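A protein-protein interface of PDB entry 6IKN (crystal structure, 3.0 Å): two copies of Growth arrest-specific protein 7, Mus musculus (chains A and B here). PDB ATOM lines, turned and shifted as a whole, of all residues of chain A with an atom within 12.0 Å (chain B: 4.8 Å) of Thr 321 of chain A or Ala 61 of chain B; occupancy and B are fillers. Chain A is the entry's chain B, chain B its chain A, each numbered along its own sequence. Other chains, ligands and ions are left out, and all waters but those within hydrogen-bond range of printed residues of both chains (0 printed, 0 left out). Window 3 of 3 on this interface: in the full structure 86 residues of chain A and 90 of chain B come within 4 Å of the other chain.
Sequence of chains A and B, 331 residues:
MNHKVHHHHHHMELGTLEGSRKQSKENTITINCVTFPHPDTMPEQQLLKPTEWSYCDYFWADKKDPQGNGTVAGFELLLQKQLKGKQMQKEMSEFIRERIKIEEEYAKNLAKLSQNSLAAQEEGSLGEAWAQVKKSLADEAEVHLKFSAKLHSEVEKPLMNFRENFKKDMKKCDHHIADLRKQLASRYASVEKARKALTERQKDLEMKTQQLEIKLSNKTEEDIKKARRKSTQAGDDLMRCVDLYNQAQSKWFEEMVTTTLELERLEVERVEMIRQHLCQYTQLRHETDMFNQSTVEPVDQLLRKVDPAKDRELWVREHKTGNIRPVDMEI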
ATOM      1  N   ARG A 312     -39.312 -24.425  27.343  1.00  0.00           N
ATOM      2  CA  ARG A 312     -37.980 -23.847  27.418  1.00  0.00           C
ATOM      3  C   ARG A 312     -36.916 -24.880  27.724  1.00  0.00           C
ATOM      4  O   ARG A 312     -35.895 -24.934  27.054  1.00  0.00           O
ATOM      5  CB  ARG A 312     -37.913 -22.769  28.491  1.00  0.00           C
ATOM      6  CG  ARG A 312     -36.588 -22.024  28.474  1.00  0.00           C
ATOM      7  CD  ARG A 312     -36.540 -20.971  29.548  1.00  0.00           C
ATOM      8  NE  ARG A 312     -36.531 -21.586  30.873  1.00  0.00           N
ATOM      9  CZ  ARG A 312     -37.501 -21.459  31.770  1.00  0.00           C
ATOM     10  NH1 ARG A 312     -38.571 -20.725  31.499  1.00  0.00           N
ATOM     11  NH2 ARG A 312     -37.398 -22.064  32.946  1.00  0.00           N
ATOM     12  N   GLU A 313     -37.146 -25.680  28.758  1.00  0.00           N
ATOM     13  CA  GLU A 313     -36.180 -26.699  29.153  1.00  0.00           C
ATOM     14  C   GLU A 313     -35.952 -27.727  28.046  1.00  0.00           C
ATOM     15  O   GLU A 313     -34.830 -28.186  27.853  1.00  0.00           O
ATOM     16  CB  GLU A 313     -36.605 -27.365  30.458  1.00  0.00           C
ATOM     17  CG  GLU A 313     -36.636 -26.371  31.606  1.00  0.00           C
ATOM     18  CD  GLU A 313     -36.368 -26.999  32.955  1.00  0.00           C
ATOM     19  OE1 GLU A 313     -36.268 -28.240  33.030  1.00  0.00           O
ATOM     20  OE2 GLU A 313     -36.258 -26.243  33.943  1.00  0.00           O
ATOM     21  N   LEU A 314     -37.015 -28.110  27.341  1.00  0.00           N
ATOM     22  CA  LEU A 314     -36.870 -29.021  26.206  1.00  0.00           C
ATOM     23  C   LEU A 314     -35.956 -28.400  25.154  1.00  0.00           C
ATOM     24  O   LEU A 314     -35.022 -29.045  24.643  1.00  0.00           O
ATOM     25  CB  LEU A 314     -38.234 -29.342  25.592  1.00  0.00           C
ATOM     26  CG  LEU A 314     -38.256 -30.389  24.476  1.00  0.00           C
ATOM     27  CD1 LEU A 314     -37.890 -31.765  25.006  1.00  0.00           C
ATOM     28  CD2 LEU A 314     -39.613 -30.416  23.790  1.00  0.00           C
ATOM     29  N   TRP A 315     -36.200 -27.118  24.887  1.00  0.00           N
ATOM     30  CA  TRP A 315     -35.462 -26.389  23.863  1.00  0.00           C
ATOM     31  C   TRP A 315     -33.991 -26.248  24.226  1.00  0.00           C
ATOM     32  O   TRP A 315     -33.116 -26.448  23.387  1.00  0.00           O
ATOM     33  CB  TRP A 315     -36.071 -25.005  23.646  1.00  0.00           C
ATOM     34  CG  TRP A 315     -35.444 -24.267  22.509  1.00  0.00           C
ATOM     35  CD1 TRP A 315     -35.780 -24.353  21.191  1.00  0.00           C
ATOM     36  CD2 TRP A 315     -34.356 -23.339  22.588  1.00  0.00           C
ATOM     37  NE1 TRP A 315     -34.973 -23.528  20.445  1.00  0.00           N
ATOM     38  CE2 TRP A 315     -34.090 -22.896  21.279  1.00  0.00           C
ATOM     39  CE3 TRP A 315     -33.582 -22.838  23.640  1.00  0.00           C
ATOM     40  CZ2 TRP A 315     -33.084 -21.975  20.994  1.00  0.00           C
ATOM     41  CZ3 TRP A 315     -32.583 -21.923  23.353  1.00  0.00           C
ATOM     42  CH2 TRP A 315     -32.345 -21.502  22.043  1.00  0.00           C
ATOM     43  N   VAL A 316     -33.729 -25.900  25.480  1.00  0.00           N
ATOM     44  CA  VAL A 316     -32.371 -25.732  25.958  1.00  0.00           C
ATOM     45  C   VAL A 316     -31.674 -27.084  25.926  1.00  0.00           C
ATOM     46  O   VAL A 316     -30.496 -27.178  25.590  1.00  0.00           O
ATOM     47  CB  VAL A 316     -32.341 -25.140  27.382  1.00  0.00           C
ATOM     48  CG1 VAL A 316     -30.945 -25.216  27.974  1.00  0.00           C
ATOM     49  CG2 VAL A 316     -32.845 -23.702  27.364  1.00  0.00           C
ATOM     50  N   ARG A 317     -32.421 -28.133  26.254  1.00  0.00           N
ATOM     51  CA  ARG A 317     -31.885 -29.489  26.212  1.00  0.00           C
ATOM     52  C   ARG A 317     -31.434 -29.860  24.801  1.00  0.00           C
ATOM     53  O   ARG A 317     -30.411 -30.527  24.634  1.00  0.00           O
ATOM     54  CB  ARG A 317     -32.920 -30.500  26.726  1.00  0.00           C
ATOM     55  CG  ARG A 317     -32.570 -31.960  26.464  1.00  0.00           C
ATOM     56  CD  ARG A 317     -33.255 -32.912  27.449  1.00  0.00           C
ATOM     57  NE  ARG A 317     -34.716 -32.866  27.383  1.00  0.00           N
ATOM     58  CZ  ARG A 317     -35.490 -32.267  28.283  1.00  0.00           C
ATOM     59  NH1 ARG A 317     -34.947 -31.665  29.331  1.00  0.00           N
ATOM     60  NH2 ARG A 317     -36.808 -32.278  28.141  1.00  0.00           N
ATOM     61  N   GLU A 318     -32.156 -29.399  23.779  1.00  0.00           N
ATOM     62  CA  GLU A 318     -31.744 -29.749  22.413  1.00  0.00           C
ATOM     63  C   GLU A 318     -30.774 -28.746  21.770  1.00  0.00           C
ATOM     64  O   GLU A 318     -30.113 -29.069  20.784  1.00  0.00           O
ATOM     65  CB  GLU A 318     -32.970 -29.942  21.504  1.00  0.00           C
ATOM     66  CG  GLU A 318     -34.090 -28.935  21.686  1.00  0.00           C
ATOM     67  CD  GLU A 318     -35.443 -29.472  21.240  1.00  0.00           C
ATOM     68  OE1 GLU A 318     -35.507 -30.643  20.807  1.00  0.00           O
ATOM     69  OE2 GLU A 318     -36.444 -28.728  21.330  1.00  0.00           O
ATOM     70  N   HIS A 319     -30.669 -27.543  22.327  1.00  0.00           N
ATOM     71  CA  HIS A 319     -29.872 -26.483  21.695  1.00  0.00           C
ATOM     72  C   HIS A 319     -28.739 -25.900  22.545  1.00  0.00           C
ATOM     73  O   HIS A 319     -28.139 -24.891  22.164  1.00  0.00           O
ATOM     74  CB  HIS A 319     -30.785 -25.346  21.235  1.00  0.00           C
ATOM     75  CG  HIS A 319     -31.549 -25.658  19.987  1.00  0.00           C
ATOM     76  ND1 HIS A 319     -32.450 -24.784  19.427  1.00  0.00           N
ATOM     77  CD2 HIS A 319     -31.522 -26.747  19.181  1.00  0.00           C
ATOM     78  CE1 HIS A 319     -32.960 -25.324  18.330  1.00  0.00           C
ATOM     79  NE2 HIS A 319     -32.413 -26.510  18.160  1.00  0.00           N
ATOM     80  N   LYS A 320     -28.452 -26.515  23.689  1.00  0.00           N
ATOM     81  CA  LYS A 320     -27.357 -26.056  24.548  1.00  0.00           C
ATOM     82  C   LYS A 320     -26.012 -26.097  23.816  1.00  0.00           C
ATOM     83  O   LYS A 320     -25.800 -26.931  22.935  1.00  0.00           O
ATOM     84  CB  LYS A 320     -27.262 -26.906  25.814  1.00  0.00           C
ATOM     85  CG  LYS A 320     -27.050 -28.384  25.545  1.00  0.00           C
ATOM     86  CD  LYS A 320     -27.042 -29.184  26.831  1.00  0.00           C
ATOM     87  CE  LYS A 320     -26.774 -30.653  26.559  1.00  0.00           C
ATOM     88  NZ  LYS A 320     -27.830 -31.243  25.695  1.00  0.00           N
ATOM     89  N   THR A 321     -25.112 -25.186  24.178  1.00  0.00           N
ATOM     90  CA  THR A 321     -23.767 -25.164  23.605  1.00  0.00           C
ATOM     91  C   THR A 321     -22.740 -25.806  24.535  1.00  0.00           C
ATOM     92  O   THR A 321     -21.612 -26.090  24.129  1.00  0.00           O
ATOM     93  CB  THR A 321     -23.314 -23.729  23.282  1.00  0.00           C
ATOM     94  OG1 THR A 321     -23.268 -22.955  24.487  1.00  0.00           O
ATOM     95  CG2 THR A 321     -24.271 -23.078  22.302  1.00  0.00           C
ATOM     96  N   GLY A 322     -23.134 -26.025  25.784  1.00  0.00           N
ATOM     97  CA  GLY A 322     -22.245 -26.613  26.767  1.00  0.00           C
ATOM     98  C   GLY A 322     -22.599 -26.146  28.163  1.00  0.00           C
ATOM     99  O   GLY A 322     -23.225 -25.099  28.333  1.00  0.00           O
ATOM    100  N   ASN A 323     -22.203 -26.922  29.166  1.00  0.00           N
ATOM    101  CA  ASN A 323     -22.624 -26.664  30.537  1.00  0.00           C
ATOM    102  C   ASN A 323     -21.492 -26.155  31.419  1.00  0.00           C
ATOM    103  O   ASN A 323     -21.563 -26.241  32.645  1.00  0.00           O
ATOM    104  CB  ASN A 323     -23.217 -27.933  31.153  1.00  0.00           C
ATOM    105  CG  ASN A 323     -22.298 -29.133  31.020  1.00  0.00           C
ATOM    106  OD1 ASN A 323     -21.109 -28.993  30.732  1.00  0.00           O
ATOM    107  ND2 ASN A 323     -22.845 -30.324  31.237  1.00  0.00           N
ATOM    108  N   ILE A 324     -20.439 -25.640  30.796  1.00  0.00           N
ATOM    109  CA  ILE A 324     -19.310 -25.119  31.555  1.00  0.00           C
ATOM    110  C   ILE A 324     -19.343 -23.596  31.629  1.00  0.00           C
ATOM    111  O   ILE A 324     -19.574 -22.917  30.630  1.00  0.00           O
ATOM    112  CB  ILE A 324     -17.976 -25.572  30.945  1.00  0.00           C
ATOM    113  CG1 ILE A 324     -17.936 -27.097  30.843  1.00  0.00           C
ATOM    114  CG2 ILE A 324     -16.810 -25.083  31.783  1.00  0.00           C
ATOM    115  CD1 ILE A 324     -18.105 -27.791  32.177  1.00  0.00           C
ATOM    116  N   ARG A 325     -19.114 -23.072  32.828  1.00  0.00           N
ATOM    117  CA  ARG A 325     -19.090 -21.636  33.063  1.00  0.00           C
ATOM    118  C   ARG A 325     -17.674 -21.113  32.849  1.00  0.00           C
ATOM    119  O   ARG A 325     -16.707 -21.844  33.059  1.00  0.00           O
ATOM    120  CB  ARG A 325     -19.579 -21.340  34.486  1.00  0.00           C
ATOM    121  CG  ARG A 325     -20.170 -19.957  34.693  1.00  0.00           C
ATOM    122  CD  ARG A 325     -20.858 -19.836  36.045  1.00  0.00           C
ATOM    123  NE  ARG A 325     -19.987 -20.221  37.152  1.00  0.00           N
ATOM    124  CZ  ARG A 325     -20.177 -21.294  37.914  1.00  0.00           C
ATOM    125  NH1 ARG A 325     -21.215 -22.090  37.692  1.00  0.00           N
ATOM    126  NH2 ARG A 325     -19.334 -21.571  38.902  1.00  0.00           N
ATOM    127  N   PRO A 326     -17.540 -19.848  32.423  1.00  0.00           N
ATOM    128  CA  PRO A 326     -16.192 -19.286  32.312  1.00  0.00           C
ATOM    129  C   PRO A 326     -15.504 -19.089  33.659  1.00  0.00           C
ATOM    130  O   PRO A 326     -16.165 -19.017  34.694  1.00  0.00           O
ATOM    131  CB  PRO A 326     -16.427 -17.934  31.629  1.00  0.00           C
ATOM    132  CG  PRO A 326     -17.740 -18.072  30.941  1.00  0.00           C
ATOM    133  CD  PRO A 326     -18.553 -18.963  31.824  1.00  0.00           C
ATOM    134  N   VAL A 327     -14.177 -19.012  33.626  1.00  0.00           N
ATOM    135  CA  VAL A 327     -13.377 -18.736  34.810  1.00  0.00           C
ATOM    136  C   VAL A 327     -12.294 -17.735  34.434  1.00  0.00           C
ATOM    137  O   VAL A 327     -12.173 -17.356  33.268  1.00  0.00           O
ATOM    138  CB  VAL A 327     -12.728 -20.009  35.390  1.00  0.00           C
ATOM    139  CG1 VAL A 327     -13.787 -20.950  35.947  1.00  0.00           C
ATOM    140  CG2 VAL A 327     -11.891 -20.707  34.335  1.00  0.00           C
ATOM    141  N   ILE B  31     -11.426 -20.636  24.114  1.00  0.00           N
ATOM    142  CA  ILE B  31     -12.070 -20.819  22.826  1.00  0.00           C
ATOM    143  C   ILE B  31     -12.899 -19.562  22.550  1.00  0.00           C
ATOM    144  O   ILE B  31     -13.697 -19.128  23.383  1.00  0.00           O
ATOM    145  CB  ILE B  31     -12.926 -22.129  22.778  1.00  0.00           C
ATOM    146  CG1 ILE B  31     -14.386 -21.900  23.177  1.00  0.00           C
ATOM    147  CG2 ILE B  31     -12.311 -23.212  23.653  1.00  0.00           C
ATOM    148  CD1 ILE B  31     -15.251 -23.145  23.125  1.00  0.00           C
ATOM    149  N   PHE B  36     -12.352 -21.069  29.776  1.00  0.00           N
ATOM    150  CA  PHE B  36     -13.037 -22.151  30.478  1.00  0.00           C
ATOM    151  C   PHE B  36     -11.976 -23.016  31.131  1.00  0.00           C
ATOM    152  O   PHE B  36     -10.818 -22.930  30.734  1.00  0.00           O
ATOM    153  CB  PHE B  36     -13.876 -22.997  29.520  1.00  0.00           C
ATOM    154  CG  PHE B  36     -14.948 -22.235  28.812  1.00  0.00           C
ATOM    155  CD1 PHE B  36     -16.159 -21.995  29.425  1.00  0.00           C
ATOM    156  CD2 PHE B  36     -14.750 -21.778  27.522  1.00  0.00           C
ATOM    157  CE1 PHE B  36     -17.152 -21.298  28.780  1.00  0.00           C
ATOM    158  CE2 PHE B  36     -15.741 -21.075  26.862  1.00  0.00           C
ATOM    159  CZ  PHE B  36     -16.946 -20.833  27.494  1.00  0.00           C
ATOM    160  N   TYR B  58     -26.315 -22.755  30.074  1.00  0.00           N
ATOM    161  CA  TYR B  58     -25.971 -23.600  28.933  1.00  0.00           C
ATOM    162  C   TYR B  58     -25.594 -22.872  27.642  1.00  0.00           C
ATOM    163  O   TYR B  58     -25.581 -23.483  26.575  1.00  0.00           O
ATOM    164  CB  TYR B  58     -27.125 -24.557  28.638  1.00  0.00           C
ATOM    165  CG  TYR B  58     -27.337 -25.601  29.711  1.00  0.00           C
ATOM    166  CD1 TYR B  58     -26.733 -26.849  29.616  1.00  0.00           C
ATOM    167  CD2 TYR B  58     -28.131 -25.340  30.819  1.00  0.00           C
ATOM    168  CE1 TYR B  58     -26.917 -27.808  30.591  1.00  0.00           C
ATOM    169  CE2 TYR B  58     -28.321 -26.296  31.800  1.00  0.00           C
ATOM    170  CZ  TYR B  58     -27.710 -27.526  31.679  1.00  0.00           C
ATOM    171  OH  TYR B  58     -27.890 -28.485  32.649  1.00  0.00           O
ATOM    172  N   PHE B  59     -25.284 -21.583  27.720  1.00  0.00           N
ATOM    173  CA  PHE B  59     -24.962 -20.840  26.504  1.00  0.00           C
ATOM    174  C   PHE B  59     -23.754 -19.916  26.656  1.00  0.00           C
ATOM    175  O   PHE B  59     -23.793 -18.757  26.249  1.00  0.00           O
ATOM    176  CB  PHE B  59     -26.180 -20.037  26.042  1.00  0.00           C
ATOM    177  CG  PHE B  59     -27.373 -20.889  25.704  1.00  0.00           C
ATOM    178  CD1 PHE B  59     -27.512 -21.445  24.440  1.00  0.00           C
ATOM    179  CD2 PHE B  59     -28.351 -21.146  26.653  1.00  0.00           C
ATOM    180  CE1 PHE B  59     -28.610 -22.236  24.128  1.00  0.00           C
ATOM    181  CE2 PHE B  59     -29.447 -21.933  26.346  1.00  0.00           C
ATOM    182  CZ  PHE B  59     -29.575 -22.478  25.083  1.00  0.00           C
ATOM    183  N   TRP B  60     -22.682 -20.432  27.246  1.00  0.00           N
ATOM    184  CA  TRP B  60     -21.447 -19.669  27.374  1.00  0.00           C
ATOM    185  C   TRP B  60     -20.535 -19.967  26.190  1.00  0.00           C
ATOM    186  O   TRP B  60     -20.018 -19.057  25.540  1.00  0.00           O
ATOM    187  CB  TRP B  60     -20.739 -19.991  28.689  1.00  0.00           C
ATOM    188  CG  TRP B  60     -21.549 -19.638  29.890  1.00  0.00           C
ATOM    189  CD1 TRP B  60     -22.180 -20.504  30.733  1.00  0.00           C
ATOM    190  CD2 TRP B  60     -21.850 -18.322  30.366  1.00  0.00           C
ATOM    191  NE1 TRP B  60     -22.840 -19.810  31.716  1.00  0.00           N
ATOM    192  CE2 TRP B  60     -22.655 -18.469  31.513  1.00  0.00           C
ATOM    193  CE3 TRP B  60     -21.510 -17.036  29.939  1.00  0.00           C
ATOM    194  CZ2 TRP B  60     -23.125 -17.376  32.239  1.00  0.00           C
ATOM    195  CZ3 TRP B  60     -21.979 -15.950  30.663  1.00  0.00           C
ATOM    196  CH2 TRP B  60     -22.778 -16.128  31.798  1.00  0.00           C
ATOM    197  N   ALA B  61     -20.349 -21.256  25.918  1.00  0.00           N
ATOM    198  CA  ALA B  61     -19.588 -21.709  24.760  1.00  0.00           C
ATOM    199  C   ALA B  61     -20.256 -21.284  23.460  1.00  0.00           C
ATOM    200  O   ALA B  61     -21.468 -21.086  23.411  1.00  0.00           O
ATOM    201  CB  ALA B  61     -19.420 -23.219  24.796  1.00  0.00           C
ATOM    202  N   ASP B  62     -19.458 -21.141  22.409  1.00  0.00           N
ATOM    203  CA  ASP B  62     -19.987 -20.854  21.082  1.00  0.00           C
ATOM    204  C   ASP B  62     -20.370 -22.152  20.377  1.00  0.00           C
ATOM    205  O   ASP B  62     -19.767 -23.196  20.626  1.00  0.00           O
ATOM    206  CB  ASP B  62     -18.958 -20.083  20.245  1.00  0.00           C
ATOM    207  CG  ASP B  62     -18.750 -18.666  20.736  1.00  0.00           C
ATOM    208  OD1 ASP B  62     -19.285 -18.321  21.810  1.00  0.00           O
ATOM    209  OD2 ASP B  62     -18.051 -17.894  20.045  1.00  0.00           O
ATOM    210  N   LYS B  63     -21.373 -22.096  19.504  1.00  0.00           N
ATOM    211  CA  LYS B  63     -21.755 -23.284  18.750  1.00  0.00           C
ATOM    212  C   LYS B  63     -20.858 -23.380  17.526  1.00  0.00           C
ATOM    213  O   LYS B  63     -20.760 -22.442  16.737  1.00  0.00           O
ATOM    214  CB  LYS B  63     -23.225 -23.249  18.328  1.00  0.00           C
ATOM    215  CG  LYS B  63     -23.686 -24.555  17.663  1.00  0.00           C
ATOM    216  CD  LYS B  63     -25.037 -24.422  16.957  1.00  0.00           C
ATOM    217  CE  LYS B  63     -24.921 -23.571  15.697  1.00  0.00           C
ATOM    218  NZ  LYS B  63     -26.229 -23.411  14.994  1.00  0.00           N
ATOM    219  N   GLY B  74     -23.696 -18.455  21.751  1.00  0.00           N
ATOM    220  CA  GLY B  74     -24.907 -19.046  22.289  1.00  0.00           C
ATOM    221  C   GLY B  74     -25.966 -17.977  22.476  1.00  0.00           C
ATOM    222  O   GLY B  74     -27.169 -18.206  22.268  1.00  0.00           O
ATOM    223  N   LEU B  77     -27.924 -17.573  19.602  1.00  0.00           N
ATOM    224  CA  LEU B  77     -28.919 -18.631  19.486  1.00  0.00           C
ATOM    225  C   LEU B  77     -30.183 -18.231  20.243  1.00  0.00           C
ATOM    226  O   LEU B  77     -31.307 -18.419  19.752  1.00  0.00           O
ATOM    227  CB  LEU B  77     -28.364 -19.950  20.022  1.00  0.00           C
ATOM    228  CG  LEU B  77     -27.367 -20.676  19.117  1.00  0.00           C
ATOM    229  CD1 LEU B  77     -26.873 -21.956  19.778  1.00  0.00           C
ATOM    230  CD2 LEU B  77     -27.963 -20.964  17.751  1.00  0.00           C
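Hydrophobic or aromatic side chains of chain B within 4 Å of the printed part of chain A: Phe 36, Tyr 58, Phe 59, Trp 60, Ala 61 and Leu 77.
The backbone carbonyl oxygen (O) of Gly 322 of chain A lies close to the backbone carbonyl oxygen (O) of Tyr 58 of chain B, at 3.4 Å.
The backbone carbonyl oxygen (O) of Tyr 58 of chain B is in hydrogen-bond range of the backbone NH (N) of Thr 321 of chain A (3.0 Å).
The backbone carbonyl oxygen (O) of Ala 61 of chain B lies within hydrogen-bond range of the side-chain hydroxyl (OG1) of Thr 321 of chain A, 2.8 Å away.
Arg 312 of chain A touches none of the printed residues of chain B.
Glu 313 of chain A touches none of the printed residues of chain B.
Of chain B, only Tyr 58 (3.0 Å), Phe 59 (3.4 Å), Trp 60 (3.8 Å), Ala 61 (2.8 Å) and Leu 77 (3.8 Å) come within 4 Å of Thr 321 of chain A.
Of the printed residues of chain B, Pro 326 of chain A touches Phe 36 (3.9 Å) and Trp 60 (3.6 Å).
Phe 59 of chain B touches just these residues of chain A: Trp 315 (3.5 Å), Val 316 (3.96 Å), His 319 (3.3 Å) and Thr 321 (3.4 Å).
Of the printed residues of chain A, Trp 60 of chain B touches Thr 321 (3.8 Å), Ile 324 (3.6 Å) and Pro 326 (3.6 Å).
Of chain A, only Thr 321 (2.8 Å) comes within 4 Å of Ala 61 of chain B.
No residue of chain A comes within 4 Å of Asp 62 of chain B.
No residue of chain A comes within 4 Å of Lys 63 of chain B.
Of the printed residues of chain A, Leu 77 of chain B touches Trp 315 (3.98 Å), His 319 (3.99 Å) and Thr 321 (3.8 Å).
The nearest residue of chain B that does not touch Thr 321 of chain A is Gly 74 of chain B (4.1 Å).
The indole nitrogen (NE1) of Trp 315 of chain A is in hydrogen-bond range of a ring nitrogen (ND1) of His 319 of chain A, at 3.0 Å.
O of Arg 317 of chain A sits at hydrogen-bond distance from NZ of Lys 320 of chain A, 2.9 Å away.
CG1 of Val 316 of chain A touches CB of Tyr 58 of chain B, at 3.9 Å.
His 319 of chain A touches Leu 77 of chain B.
CD1 of Tyr 58 of chain B touches CD of Lys 320 of chain A, 3.6 Å away.
CA of Phe 59 of chain B touches OG1 of Thr 321 of chain A (3.4 Å).
N of Trp 60 of chain B touches OG1 of Thr 321 of chain A (3.8 Å).
O of Ile 324 of chain A touches CE1 of Phe 36 of chain B, 3.5 Å away.
Ile 324 of chain A touches Trp 60 of chain B.
Arg 325 of chain A touches Phe 36 of chain B (O to CD1, 3.7 Å).
CE1 of Phe 36 of chain B touches CG of Pro 326 of chain A, 3.9 Å away.
Trp 60 of chain B touches Pro 326 of chain A.
No position is printed for both chains.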
